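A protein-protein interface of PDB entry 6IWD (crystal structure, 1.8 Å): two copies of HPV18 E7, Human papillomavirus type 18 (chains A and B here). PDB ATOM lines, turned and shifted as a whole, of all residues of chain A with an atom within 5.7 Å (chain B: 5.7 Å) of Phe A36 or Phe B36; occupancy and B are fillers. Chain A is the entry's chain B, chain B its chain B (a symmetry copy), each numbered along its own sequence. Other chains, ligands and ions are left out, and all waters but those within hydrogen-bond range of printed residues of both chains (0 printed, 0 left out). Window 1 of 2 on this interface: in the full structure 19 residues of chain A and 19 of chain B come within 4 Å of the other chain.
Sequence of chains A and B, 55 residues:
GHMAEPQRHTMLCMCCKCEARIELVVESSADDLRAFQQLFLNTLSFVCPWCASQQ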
ATOM      1  N   MET A  11      -1.289  -8.597  23.253  1.00  0.00           N
ATOM      2  CA  MET A  11      -0.105  -9.228  23.822  1.00  0.00           C
ATOM      3  C   MET A  11      -0.455  -9.776  25.198  1.00  0.00           C
ATOM      4  O   MET A  11      -0.818  -9.010  26.097  1.00  0.00           O
ATOM      5  CB  MET A  11       1.049  -8.235  23.935  1.00  0.00           C
ATOM      6  CG  MET A  11       1.561  -7.703  22.612  1.00  0.00           C
ATOM      7  SD  MET A  11       2.666  -8.865  21.790  1.00  0.00           S
ATOM      8  CE  MET A  11       3.876  -9.151  23.080  1.00  0.00           C
ATOM      9  N   LEU A  24      -2.281  -6.787  27.144  1.00  0.00           N
ATOM     10  CA  LEU A  24      -1.989  -5.488  26.546  1.00  0.00           C
ATOM     11  C   LEU A  24      -2.565  -5.454  25.140  1.00  0.00           C
ATOM     12  O   LEU A  24      -2.366  -6.392  24.361  1.00  0.00           O
ATOM     13  CB  LEU A  24      -0.487  -5.219  26.491  1.00  0.00           C
ATOM     14  CG  LEU A  24       0.293  -5.299  27.792  1.00  0.00           C
ATOM     15  CD1 LEU A  24       1.765  -5.177  27.494  1.00  0.00           C
ATOM     16  CD2 LEU A  24      -0.166  -4.201  28.736  1.00  0.00           C
ATOM     17  N   VAL A  26      -2.631  -3.239  21.702  1.00  0.00           N
ATOM     18  CA  VAL A  26      -1.932  -2.186  20.986  1.00  0.00           C
ATOM     19  C   VAL A  26      -2.484  -2.075  19.568  1.00  0.00           C
ATOM     20  O   VAL A  26      -3.120  -2.990  19.038  1.00  0.00           O
ATOM     21  CB  VAL A  26      -0.404  -2.426  20.951  1.00  0.00           C
ATOM     22  CG1 VAL A  26       0.177  -2.347  22.356  1.00  0.00           C
ATOM     23  CG2 VAL A  26      -0.084  -3.773  20.319  1.00  0.00           C
ATOM     24  N   ASP A  31       6.003  -4.183  11.760  1.00  0.00           N
ATOM     25  CA  ASP A  31       7.392  -4.067  12.202  1.00  0.00           C
ATOM     26  C   ASP A  31       7.481  -3.623  13.655  1.00  0.00           C
ATOM     27  O   ASP A  31       8.347  -4.101  14.403  1.00  0.00           O
ATOM     28  CB  ASP A  31       8.167  -3.092  11.319  1.00  0.00           C
ATOM     29  CG  ASP A  31       8.466  -3.650   9.942  1.00  0.00           C
ATOM     30  OD1 ASP A  31       8.275  -4.869   9.719  1.00  0.00           O
ATOM     31  OD2 ASP A  31       8.906  -2.856   9.082  1.00  0.00           O
ATOM     32  N   ASP A  32       6.626  -2.684  14.072  1.00  0.00           N
ATOM     33  CA  ASP A  32       6.702  -2.245  15.465  1.00  0.00           C
ATOM     34  C   ASP A  32       6.162  -3.314  16.408  1.00  0.00           C
ATOM     35  O   ASP A  32       6.630  -3.434  17.547  1.00  0.00           O
ATOM     36  CB  ASP A  32       5.959  -0.919  15.658  1.00  0.00           C
ATOM     37  CG  ASP A  32       6.718   0.283  15.065  1.00  0.00           C
ATOM     38  OD1 ASP A  32       7.974   0.268  14.999  1.00  0.00           O
ATOM     39  OD2 ASP A  32       6.048   1.259  14.661  1.00  0.00           O
ATOM     40  N   LEU A  33       5.207  -4.123  15.941  1.00  0.00           N
ATOM     41  CA  LEU A  33       4.753  -5.256  16.736  1.00  0.00           C
ATOM     42  C   LEU A  33       5.892  -6.243  16.967  1.00  0.00           C
ATOM     43  O   LEU A  33       6.105  -6.706  18.091  1.00  0.00           O
ATOM     44  CB  LEU A  33       3.563  -5.943  16.055  1.00  0.00           C
ATOM     45  CG  LEU A  33       3.175  -7.268  16.728  1.00  0.00           C
ATOM     46  CD1 LEU A  33       2.713  -7.054  18.153  1.00  0.00           C
ATOM     47  CD2 LEU A  33       2.103  -8.010  15.934  1.00  0.00           C
ATOM     48  N   ARG A  34       6.637  -6.584  15.907  1.00  0.00           N
ATOM     49  CA  ARG A  34       7.758  -7.514  16.064  1.00  0.00           C
ATOM     50  C   ARG A  34       8.801  -6.949  17.016  1.00  0.00           C
ATOM     51  O   ARG A  34       9.331  -7.672  17.872  1.00  0.00           O
ATOM     52  CB  ARG A  34       8.403  -7.809  14.706  1.00  0.00           C
ATOM     53  CG  ARG A  34       9.368  -8.983  14.737  1.00  0.00           C
ATOM     54  CD  ARG A  34       8.591 -10.271  14.853  1.00  0.00           C
ATOM     55  NE  ARG A  34       7.966 -10.588  13.575  1.00  0.00           N
ATOM     56  CZ  ARG A  34       6.825 -11.256  13.425  1.00  0.00           C
ATOM     57  NH1 ARG A  34       6.124 -11.671  14.474  1.00  0.00           N
ATOM     58  NH2 ARG A  34       6.372 -11.475  12.207  1.00  0.00           N
ATOM     59  N   ALA A  35       9.104  -5.653  16.880  1.00  0.00           N
ATOM     60  CA  ALA A  35      10.082  -5.024  17.762  1.00  0.00           C
ATOM     61  C   ALA A  35       9.640  -5.091  19.219  1.00  0.00           C
ATOM     62  O   ALA A  35      10.462  -5.304  20.120  1.00  0.00           O
ATOM     63  CB  ALA A  35      10.309  -3.576  17.327  1.00  0.00           C
ATOM     64  N   PHE A  36       8.341  -4.894  19.466  1.00  0.00           N
ATOM     65  CA  PHE A  36       7.776  -4.982  20.809  1.00  0.00           C
ATOM     66  C   PHE A  36       7.863  -6.407  21.354  1.00  0.00           C
ATOM     67  O   PHE A  36       8.264  -6.617  22.507  1.00  0.00           O
ATOM     68  CB  PHE A  36       6.326  -4.485  20.755  1.00  0.00           C
ATOM     69  CG  PHE A  36       5.637  -4.365  22.098  1.00  0.00           C
ATOM     70  CD1 PHE A  36       6.306  -3.908  23.219  1.00  0.00           C
ATOM     71  CD2 PHE A  36       4.279  -4.644  22.204  1.00  0.00           C
ATOM     72  CE1 PHE A  36       5.641  -3.791  24.449  1.00  0.00           C
ATOM     73  CE2 PHE A  36       3.613  -4.517  23.421  1.00  0.00           C
ATOM     74  CZ  PHE A  36       4.291  -4.087  24.538  1.00  0.00           C
ATOM     75  N   GLN A  37       7.497  -7.400  20.533  1.00  0.00           N
ATOM     76  CA  GLN A  37       7.680  -8.806  20.906  1.00  0.00           C
ATOM     77  C   GLN A  37       9.131  -9.090  21.299  1.00  0.00           C
ATOM     78  O   GLN A  37       9.398  -9.716  22.330  1.00  0.00           O
ATOM     79  CB  GLN A  37       7.233  -9.707  19.742  1.00  0.00           C
ATOM     80  CG  GLN A  37       5.728  -9.698  19.489  1.00  0.00           C
ATOM     81  CD  GLN A  37       5.334 -10.389  18.185  1.00  0.00           C
ATOM     82  OE1 GLN A  37       6.122 -10.464  17.236  1.00  0.00           O
ATOM     83  NE2 GLN A  37       4.101 -10.894  18.135  1.00  0.00           N
ATOM     84  N   GLN A  38      10.087  -8.597  20.503  1.00  0.00           N
ATOM     85  CA  GLN A  38      11.499  -8.843  20.796  1.00  0.00           C
ATOM     86  C   GLN A  38      11.910  -8.271  22.157  1.00  0.00           C
ATOM     87  O   GLN A  38      12.756  -8.861  22.846  1.00  0.00           O
ATOM     88  CB  GLN A  38      12.365  -8.265  19.666  1.00  0.00           C
ATOM     89  CG  GLN A  38      13.873  -8.491  19.831  1.00  0.00           C
ATOM     90  CD  GLN A  38      14.239  -9.971  19.920  1.00  0.00           C
ATOM     91  OE1 GLN A  38      13.847 -10.764  19.077  1.00  0.00           O
ATOM     92  NE2 GLN A  38      14.989 -10.342  20.951  1.00  0.00           N
ATOM     93  N   LEU A  39      11.301  -7.156  22.579  1.00  0.00           N
ATOM     94  CA  LEU A  39      11.656  -6.581  23.880  1.00  0.00           C
ATOM     95  C   LEU A  39      11.318  -7.532  25.023  1.00  0.00           C
ATOM     96  O   LEU A  39      12.050  -7.593  26.017  1.00  0.00           O
ATOM     97  CB  LEU A  39      10.960  -5.228  24.074  1.00  0.00           C
ATOM     98  CG  LEU A  39      11.413  -4.136  23.104  1.00  0.00           C
ATOM     99  CD1 LEU A  39      10.797  -2.761  23.442  1.00  0.00           C
ATOM    100  CD2 LEU A  39      12.931  -4.055  23.085  1.00  0.00           C
ATOM    101  N   PHE A  40      10.212  -8.288  24.903  1.00  0.00           N
ATOM    102  CA  PHE A  40       9.885  -9.289  25.920  1.00  0.00           C
ATOM    103  C   PHE A  40      10.926 -10.392  25.972  1.00  0.00           C
ATOM    104  O   PHE A  40      11.083 -11.053  27.006  1.00  0.00           O
ATOM    105  CB  PHE A  40       8.509  -9.915  25.650  1.00  0.00           C
ATOM    106  CG  PHE A  40       7.347  -9.021  25.988  1.00  0.00           C
ATOM    107  CD1 PHE A  40       6.840  -8.136  25.045  1.00  0.00           C
ATOM    108  CD2 PHE A  40       6.749  -9.079  27.237  1.00  0.00           C
ATOM    109  CE1 PHE A  40       5.761  -7.311  25.352  1.00  0.00           C
ATOM    110  CE2 PHE A  40       5.672  -8.258  27.546  1.00  0.00           C
ATOM    111  CZ  PHE A  40       5.182  -7.379  26.610  1.00  0.00           C
ATOM    112  N   LEU A  44      12.437  -6.637  28.880  1.00  0.00           N
ATOM    113  CA  LEU A  44      11.244  -5.851  29.189  1.00  0.00           C
ATOM    114  C   LEU A  44      10.170  -6.740  29.807  1.00  0.00           C
ATOM    115  O   LEU A  44       9.785  -7.757  29.225  1.00  0.00           O
ATOM    116  CB  LEU A  44      10.713  -5.172  27.931  1.00  0.00           C
ATOM    117  CG  LEU A  44       9.451  -4.307  28.068  1.00  0.00           C
ATOM    118  CD1 LEU A  44       9.804  -3.035  28.820  1.00  0.00           C
ATOM    119  CD2 LEU A  44       8.824  -3.959  26.704  1.00  0.00           C
ATOM    120  N   PHE A  46       6.356  -6.385  32.287  1.00  0.00           N
ATOM    121  CA  PHE A  46       5.311  -5.510  32.794  1.00  0.00           C
ATOM    122  C   PHE A  46       4.915  -5.882  34.217  1.00  0.00           C
ATOM    123  O   PHE A  46       5.000  -7.043  34.627  1.00  0.00           O
ATOM    124  CB  PHE A  46       4.084  -5.544  31.883  1.00  0.00           C
ATOM    125  CG  PHE A  46       4.262  -4.741  30.641  1.00  0.00           C
ATOM    126  CD1 PHE A  46       5.003  -5.245  29.580  1.00  0.00           C
ATOM    127  CD2 PHE A  46       3.733  -3.458  30.548  1.00  0.00           C
ATOM    128  CE1 PHE A  46       5.199  -4.487  28.433  1.00  0.00           C
ATOM    129  CE2 PHE A  46       3.911  -2.701  29.406  1.00  0.00           C
ATOM    130  CZ  PHE A  46       4.644  -3.213  28.340  1.00  0.00           C
ATOM    131  N   MET B  11       5.678   4.496  32.194  1.00  0.00           N
ATOM    132  CA  MET B  11       5.425   5.125  30.904  1.00  0.00           C
ATOM    133  C   MET B  11       4.007   5.678  30.899  1.00  0.00           C
ATOM    134  O   MET B  11       3.043   4.916  31.028  1.00  0.00           O
ATOM    135  CB  MET B  11       5.599   4.128  29.761  1.00  0.00           C
ATOM    136  CG  MET B  11       7.006   3.591  29.597  1.00  0.00           C
ATOM    137  SD  MET B  11       8.083   4.747  28.729  1.00  0.00           S
ATOM    138  CE  MET B  11       7.136   5.032  27.234  1.00  0.00           C
ATOM    139  N   LEU B  24       1.656   2.701  32.190  1.00  0.00           N
ATOM    140  CA  LEU B  24       2.303   1.400  32.060  1.00  0.00           C
ATOM    141  C   LEU B  24       3.521   1.364  32.968  1.00  0.00           C
ATOM    142  O   LEU B  24       4.329   2.299  32.967  1.00  0.00           O
ATOM    143  CB  LEU B  24       2.731   1.125  30.619  1.00  0.00           C
ATOM    144  CG  LEU B  24       1.665   1.206  29.540  1.00  0.00           C
ATOM    145  CD1 LEU B  24       2.321   1.078  28.189  1.00  0.00           C
ATOM    146  CD2 LEU B  24       0.633   0.112  29.751  1.00  0.00           C
ATOM    147  N   VAL B  26       6.826  -0.860  33.896  1.00  0.00           N
ATOM    148  CA  VAL B  26       7.690  -1.918  33.401  1.00  0.00           C
ATOM    149  C   VAL B  26       8.925  -2.031  34.289  1.00  0.00           C
ATOM    150  O   VAL B  26       9.282  -1.115  35.034  1.00  0.00           O
ATOM    151  CB  VAL B  26       8.106  -1.684  31.929  1.00  0.00           C
ATOM    152  CG1 VAL B  26       6.890  -1.761  31.016  1.00  0.00           C
ATOM    153  CG2 VAL B  26       8.803  -0.339  31.773  1.00  0.00           C
ATOM    154  N   ASP B  31      18.611   0.026  28.013  1.00  0.00           N
ATOM    155  CA  ASP B  31      18.530  -0.094  26.558  1.00  0.00           C
ATOM    156  C   ASP B  31      17.143  -0.535  26.110  1.00  0.00           C
ATOM    157  O   ASP B  31      16.636  -0.058  25.084  1.00  0.00           O
ATOM    158  CB  ASP B  31      19.574  -1.074  26.030  1.00  0.00           C
ATOM    159  CG  ASP B  31      20.984  -0.522  26.084  1.00  0.00           C
ATOM    160  OD1 ASP B  31      21.157   0.697  26.321  1.00  0.00           O
ATOM    161  OD2 ASP B  31      21.924  -1.319  25.874  1.00  0.00           O
ATOM    162  N   ASP B  32      16.523  -1.470  26.837  1.00  0.00           N
ATOM    163  CA  ASP B  32      15.191  -1.905  26.418  1.00  0.00           C
ATOM    164  C   ASP B  32      14.147  -0.831  26.703  1.00  0.00           C
ATOM    165  O   ASP B  32      13.161  -0.710  25.964  1.00  0.00           O
ATOM    166  CB  ASP B  32      14.814  -3.228  27.092  1.00  0.00           C
ATOM    167  CG  ASP B  32      15.574  -4.434  26.508  1.00  0.00           C
ATOM    168  OD1 ASP B  32      15.951  -4.423  25.309  1.00  0.00           O
ATOM    169  OD2 ASP B  32      15.794  -5.408  27.261  1.00  0.00           O
ATOM    170  N   LEU B  33      14.363  -0.020  27.741  1.00  0.00           N
ATOM    171  CA  LEU B  33      13.485   1.117  27.980  1.00  0.00           C
ATOM    172  C   LEU B  33      13.548   2.100  26.816  1.00  0.00           C
ATOM    173  O   LEU B  33      12.515   2.566  26.327  1.00  0.00           O
ATOM    174  CB  LEU B  33      13.850   1.806  29.300  1.00  0.00           C
ATOM    175  CG  LEU B  33      13.106   3.134  29.504  1.00  0.00           C
ATOM    176  CD1 LEU B  33      11.609   2.926  29.596  1.00  0.00           C
ATOM    177  CD2 LEU B  33      13.609   3.878  30.738  1.00  0.00           C
ATOM    178  N   ARG B  34      14.762   2.435  26.359  1.00  0.00           N
ATOM    179  CA  ARG B  34      14.893   3.362  25.231  1.00  0.00           C
ATOM    180  C   ARG B  34      14.229   2.796  23.985  1.00  0.00           C
ATOM    181  O   ARG B  34      13.535   3.519  23.256  1.00  0.00           O
ATOM    182  CB  ARG B  34      16.370   3.651  24.945  1.00  0.00           C
ATOM    183  CG  ARG B  34      16.585   4.821  23.999  1.00  0.00           C
ATOM    184  CD  ARG B  34      16.284   6.112  24.719  1.00  0.00           C
ATOM    185  NE  ARG B  34      17.366   6.428  25.642  1.00  0.00           N
ATOM    186  CZ  ARG B  34      17.229   7.100  26.782  1.00  0.00           C
ATOM    187  NH1 ARG B  34      16.040   7.520  27.198  1.00  0.00           N
ATOM    188  NH2 ARG B  34      18.297   7.317  27.525  1.00  0.00           N
ATOM    189  N   ALA B  35      14.432   1.499  23.729  1.00  0.00           N
ATOM    190  CA  ALA B  35      13.819   0.869  22.563  1.00  0.00           C
ATOM    191  C   ALA B  35      12.298   0.941  22.628  1.00  0.00           C
ATOM    192  O   ALA B  35      11.633   1.153  21.606  1.00  0.00           O
ATOM    193  CB  ALA B  35      14.293  -0.582  22.456  1.00  0.00           C
ATOM    194  N   PHE B  36      11.735   0.749  23.824  1.00  0.00           N
ATOM    195  CA  PHE B  36      10.293   0.842  24.036  1.00  0.00           C
ATOM    196  C   PHE B  36       9.792   2.269  23.812  1.00  0.00           C
ATOM    197  O   PHE B  36       8.777   2.481  23.136  1.00  0.00           O
ATOM    198  CB  PHE B  36       9.982   0.351  25.455  1.00  0.00           C
ATOM    199  CG  PHE B  36       8.509   0.237  25.788  1.00  0.00           C
ATOM    200  CD1 PHE B  36       7.589  -0.219  24.862  1.00  0.00           C
ATOM    201  CD2 PHE B  36       8.069   0.521  27.075  1.00  0.00           C
ATOM    202  CE1 PHE B  36       6.232  -0.330  25.198  1.00  0.00           C
ATOM    203  CE2 PHE B  36       6.724   0.400  27.418  1.00  0.00           C
ATOM    204  CZ  PHE B  36       5.810  -0.029  26.483  1.00  0.00           C
ATOM    205  N   GLN B  37      10.500   3.261  24.368  1.00  0.00           N
ATOM    206  CA  GLN B  37      10.189   4.668  24.095  1.00  0.00           C
ATOM    207  C   GLN B  37      10.172   4.948  22.591  1.00  0.00           C
ATOM    208  O   GLN B  37       9.243   5.575  22.073  1.00  0.00           O
ATOM    209  CB  GLN B  37      11.208   5.567  24.815  1.00  0.00           C
ATOM    210  CG  GLN B  37      11.077   5.562  26.336  1.00  0.00           C
ATOM    211  CD  GLN B  37      12.244   6.251  27.041  1.00  0.00           C
ATOM    212  OE1 GLN B  37      13.361   6.321  26.514  1.00  0.00           O
ATOM    213  NE2 GLN B  37      11.987   6.760  28.246  1.00  0.00           N
ATOM    214  N   GLN B  38      11.179   4.449  21.865  1.00  0.00           N
ATOM    215  CA  GLN B  38      11.249   4.691  20.424  1.00  0.00           C
ATOM    216  C   GLN B  38      10.032   4.121  19.688  1.00  0.00           C
ATOM    217  O   GLN B  38       9.578   4.709  18.695  1.00  0.00           O
ATOM    218  CB  GLN B  38      12.558   4.106  19.869  1.00  0.00           C
ATOM    219  CG  GLN B  38      12.775   4.327  18.367  1.00  0.00           C
ATOM    220  CD  GLN B  38      12.785   5.807  17.986  1.00  0.00           C
ATOM    221  OE1 GLN B  38      13.507   6.598  18.573  1.00  0.00           O
ATOM    222  NE2 GLN B  38      11.975   6.177  17.002  1.00  0.00           N
ATOM    223  N   LEU B  39       9.467   3.009  20.175  1.00  0.00           N
ATOM    224  CA  LEU B  39       8.294   2.436  19.508  1.00  0.00           C
ATOM    225  C   LEU B  39       7.106   3.392  19.548  1.00  0.00           C
ATOM    226  O   LEU B  39       6.326   3.453  18.591  1.00  0.00           O
ATOM    227  CB  LEU B  39       7.927   1.087  20.138  1.00  0.00           C
ATOM    228  CG  LEU B  39       8.975  -0.010  19.944  1.00  0.00           C
ATOM    229  CD1 LEU B  39       8.490  -1.382  20.460  1.00  0.00           C
ATOM    230  CD2 LEU B  39       9.372  -0.097  18.479  1.00  0.00           C
ATOM    231  N   PHE B  40       6.949   4.151  20.647  1.00  0.00           N
ATOM    232  CA  PHE B  40       5.886   5.156  20.707  1.00  0.00           C
ATOM    233  C   PHE B  40       6.099   6.256  19.683  1.00  0.00           C
ATOM    234  O   PHE B  40       5.139   6.919  19.271  1.00  0.00           O
ATOM    235  CB  PHE B  40       5.806   5.786  22.105  1.00  0.00           C
ATOM    236  CG  PHE B  40       5.186   4.897  23.148  1.00  0.00           C
ATOM    237  CD1 PHE B  40       5.969   4.011  23.877  1.00  0.00           C
ATOM    238  CD2 PHE B  40       3.828   4.961  23.416  1.00  0.00           C
ATOM    239  CE1 PHE B  40       5.400   3.191  24.847  1.00  0.00           C
ATOM    240  CE2 PHE B  40       3.256   4.145  24.384  1.00  0.00           C
ATOM    241  CZ  PHE B  40       4.038   3.265  25.094  1.00  0.00           C
ATOM    242  N   LEU B  44       3.647   2.504  17.504  1.00  0.00           N
ATOM    243  CA  LEU B  44       3.047   1.723  18.584  1.00  0.00           C
ATOM    244  C   LEU B  44       2.184   2.617  19.468  1.00  0.00           C
ATOM    245  O   LEU B  44       2.655   3.634  19.983  1.00  0.00           O
ATOM    246  CB  LEU B  44       4.130   1.043  19.414  1.00  0.00           C
ATOM    247  CG  LEU B  44       3.680   0.182  20.604  1.00  0.00           C
ATOM    248  CD1 LEU B  44       3.035  -1.089  20.079  1.00  0.00           C
ATOM    249  CD2 LEU B  44       4.843  -0.168  21.553  1.00  0.00           C
ATOM    250  N   PHE B  46      -1.170   2.283  22.543  1.00  0.00           N
ATOM    251  CA  PHE B  46      -1.925   1.413  23.432  1.00  0.00           C
ATOM    252  C   PHE B  46      -3.401   1.790  23.459  1.00  0.00           C
ATOM    253  O   PHE B  46      -3.772   2.952  23.271  1.00  0.00           O
ATOM    254  CB  PHE B  46      -1.349   1.449  24.846  1.00  0.00           C
ATOM    255  CG  PHE B  46      -0.105   0.641  24.986  1.00  0.00           C
ATOM    256  CD1 PHE B  46       1.109   1.139  24.532  1.00  0.00           C
ATOM    257  CD2 PHE B  46      -0.152  -0.640  25.525  1.00  0.00           C
ATOM    258  CE1 PHE B  46       2.267   0.378  24.631  1.00  0.00           C
ATOM    259  CE2 PHE B  46       0.997  -1.401  25.640  1.00  0.00           C
ATOM    260  CZ  PHE B  46       2.213  -0.894  25.195  1.00  0.00           C
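Among the printed residues, pairs that only touch across the chains: Phe A46 with Val B26 (3.5 Å), Val A26 with Phe B46 (3.5 Å), Phe A36 with Phe B36 (3.6 Å), Phe A36 with Leu B39 (3.7 Å), Leu A39 with Phe B36 (3.7 Å), Asp A32 with Leu B39 (3.8 Å), Leu A39 with Asp B32 (3.8 Å), Ala A35 with Leu B39 (3.8 Å), Leu A39 with Ala B35 (3.8 Å), Leu A44 with Val B26 (3.8 Å), Val A26 with Leu B44 (3.8 Å), Phe A36 with Phe B46 (3.9 Å), Phe A46 with Phe B36 (3.9 Å), Asp A32 with Leu B44 (3.9 Å) and Leu A44 with Asp B32 (3.9 Å).
Hydrophobic or aromatic side chains of chain A that line the printed part of chain B: Val A26, Ala A35, Phe A36, Leu A39, Leu A44 and Phe A46. Of the 15 printed residues of chain B, 7 touch a printed residue of chain A. Hydrophobic or aromatic side chains of chain B that line the printed part of chain A: Val B26, Ala B35, Phe B36, Leu B39, Leu B44 and Phe B46. Among the printed residues, 15 pairs touch across the chains. Among the printed residues, no Asp or Glu carboxylate lies within 4 Å of a Lys or Arg side-chain nitrogen of the other chain.
Val A26 touches Phe B46, and with the chains exchanged Phe A46 touches Val B26. Asp A32 touches Leu B39, and with the chains exchanged Leu A39 touches Asp B32. Phe B36 touches its own counterpart, Phe A36. Phe A36 touches Leu B39, and with the chains exchanged Leu A39 touches Phe B36. Positions printed for both chains: 11, 24, 26, 31, 32, 33, 34, 35, 36, 37, 38, 39, 40, 44 and 46. Of the 15 pairs that touch across the chains among the printed residues, 15 have their exchanged pair printed and touching as well.
The backbone carbonyl oxygen (O) of Leu A39 sits at hydrogen-bond distance from the backbone NH (N) of Leu A44, 3.0 Å away. N of Leu B44 is in hydrogen-bond range of O of Leu B39, at 3.0 Å.
Of the printed residues of chain B, Asp A32 touches Leu B39 (3.8 Å) and Leu B44 (3.9 Å). Printed residues of chain B within 4 Å of Leu A39: Asp B32 (3.8 Å), Ala B35 (3.8 Å) and Phe B36 (3.7 Å). Phe A40 touches none of the printed residues of chain B. Of the printed residues of chain B, Phe A46 touches Val B26 (3.5 Å) and Phe B36 (3.9 Å). Of the printed residues of chain A, Asp B32 touches Leu A39 and Leu A44. Arg B34 touches none of the printed residues of chain A. Of chain A, only Phe A36 (3.6 Å), Leu A39 (3.7 Å) and Phe A46 (3.9 Å) come within 4 Å of Phe B36.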
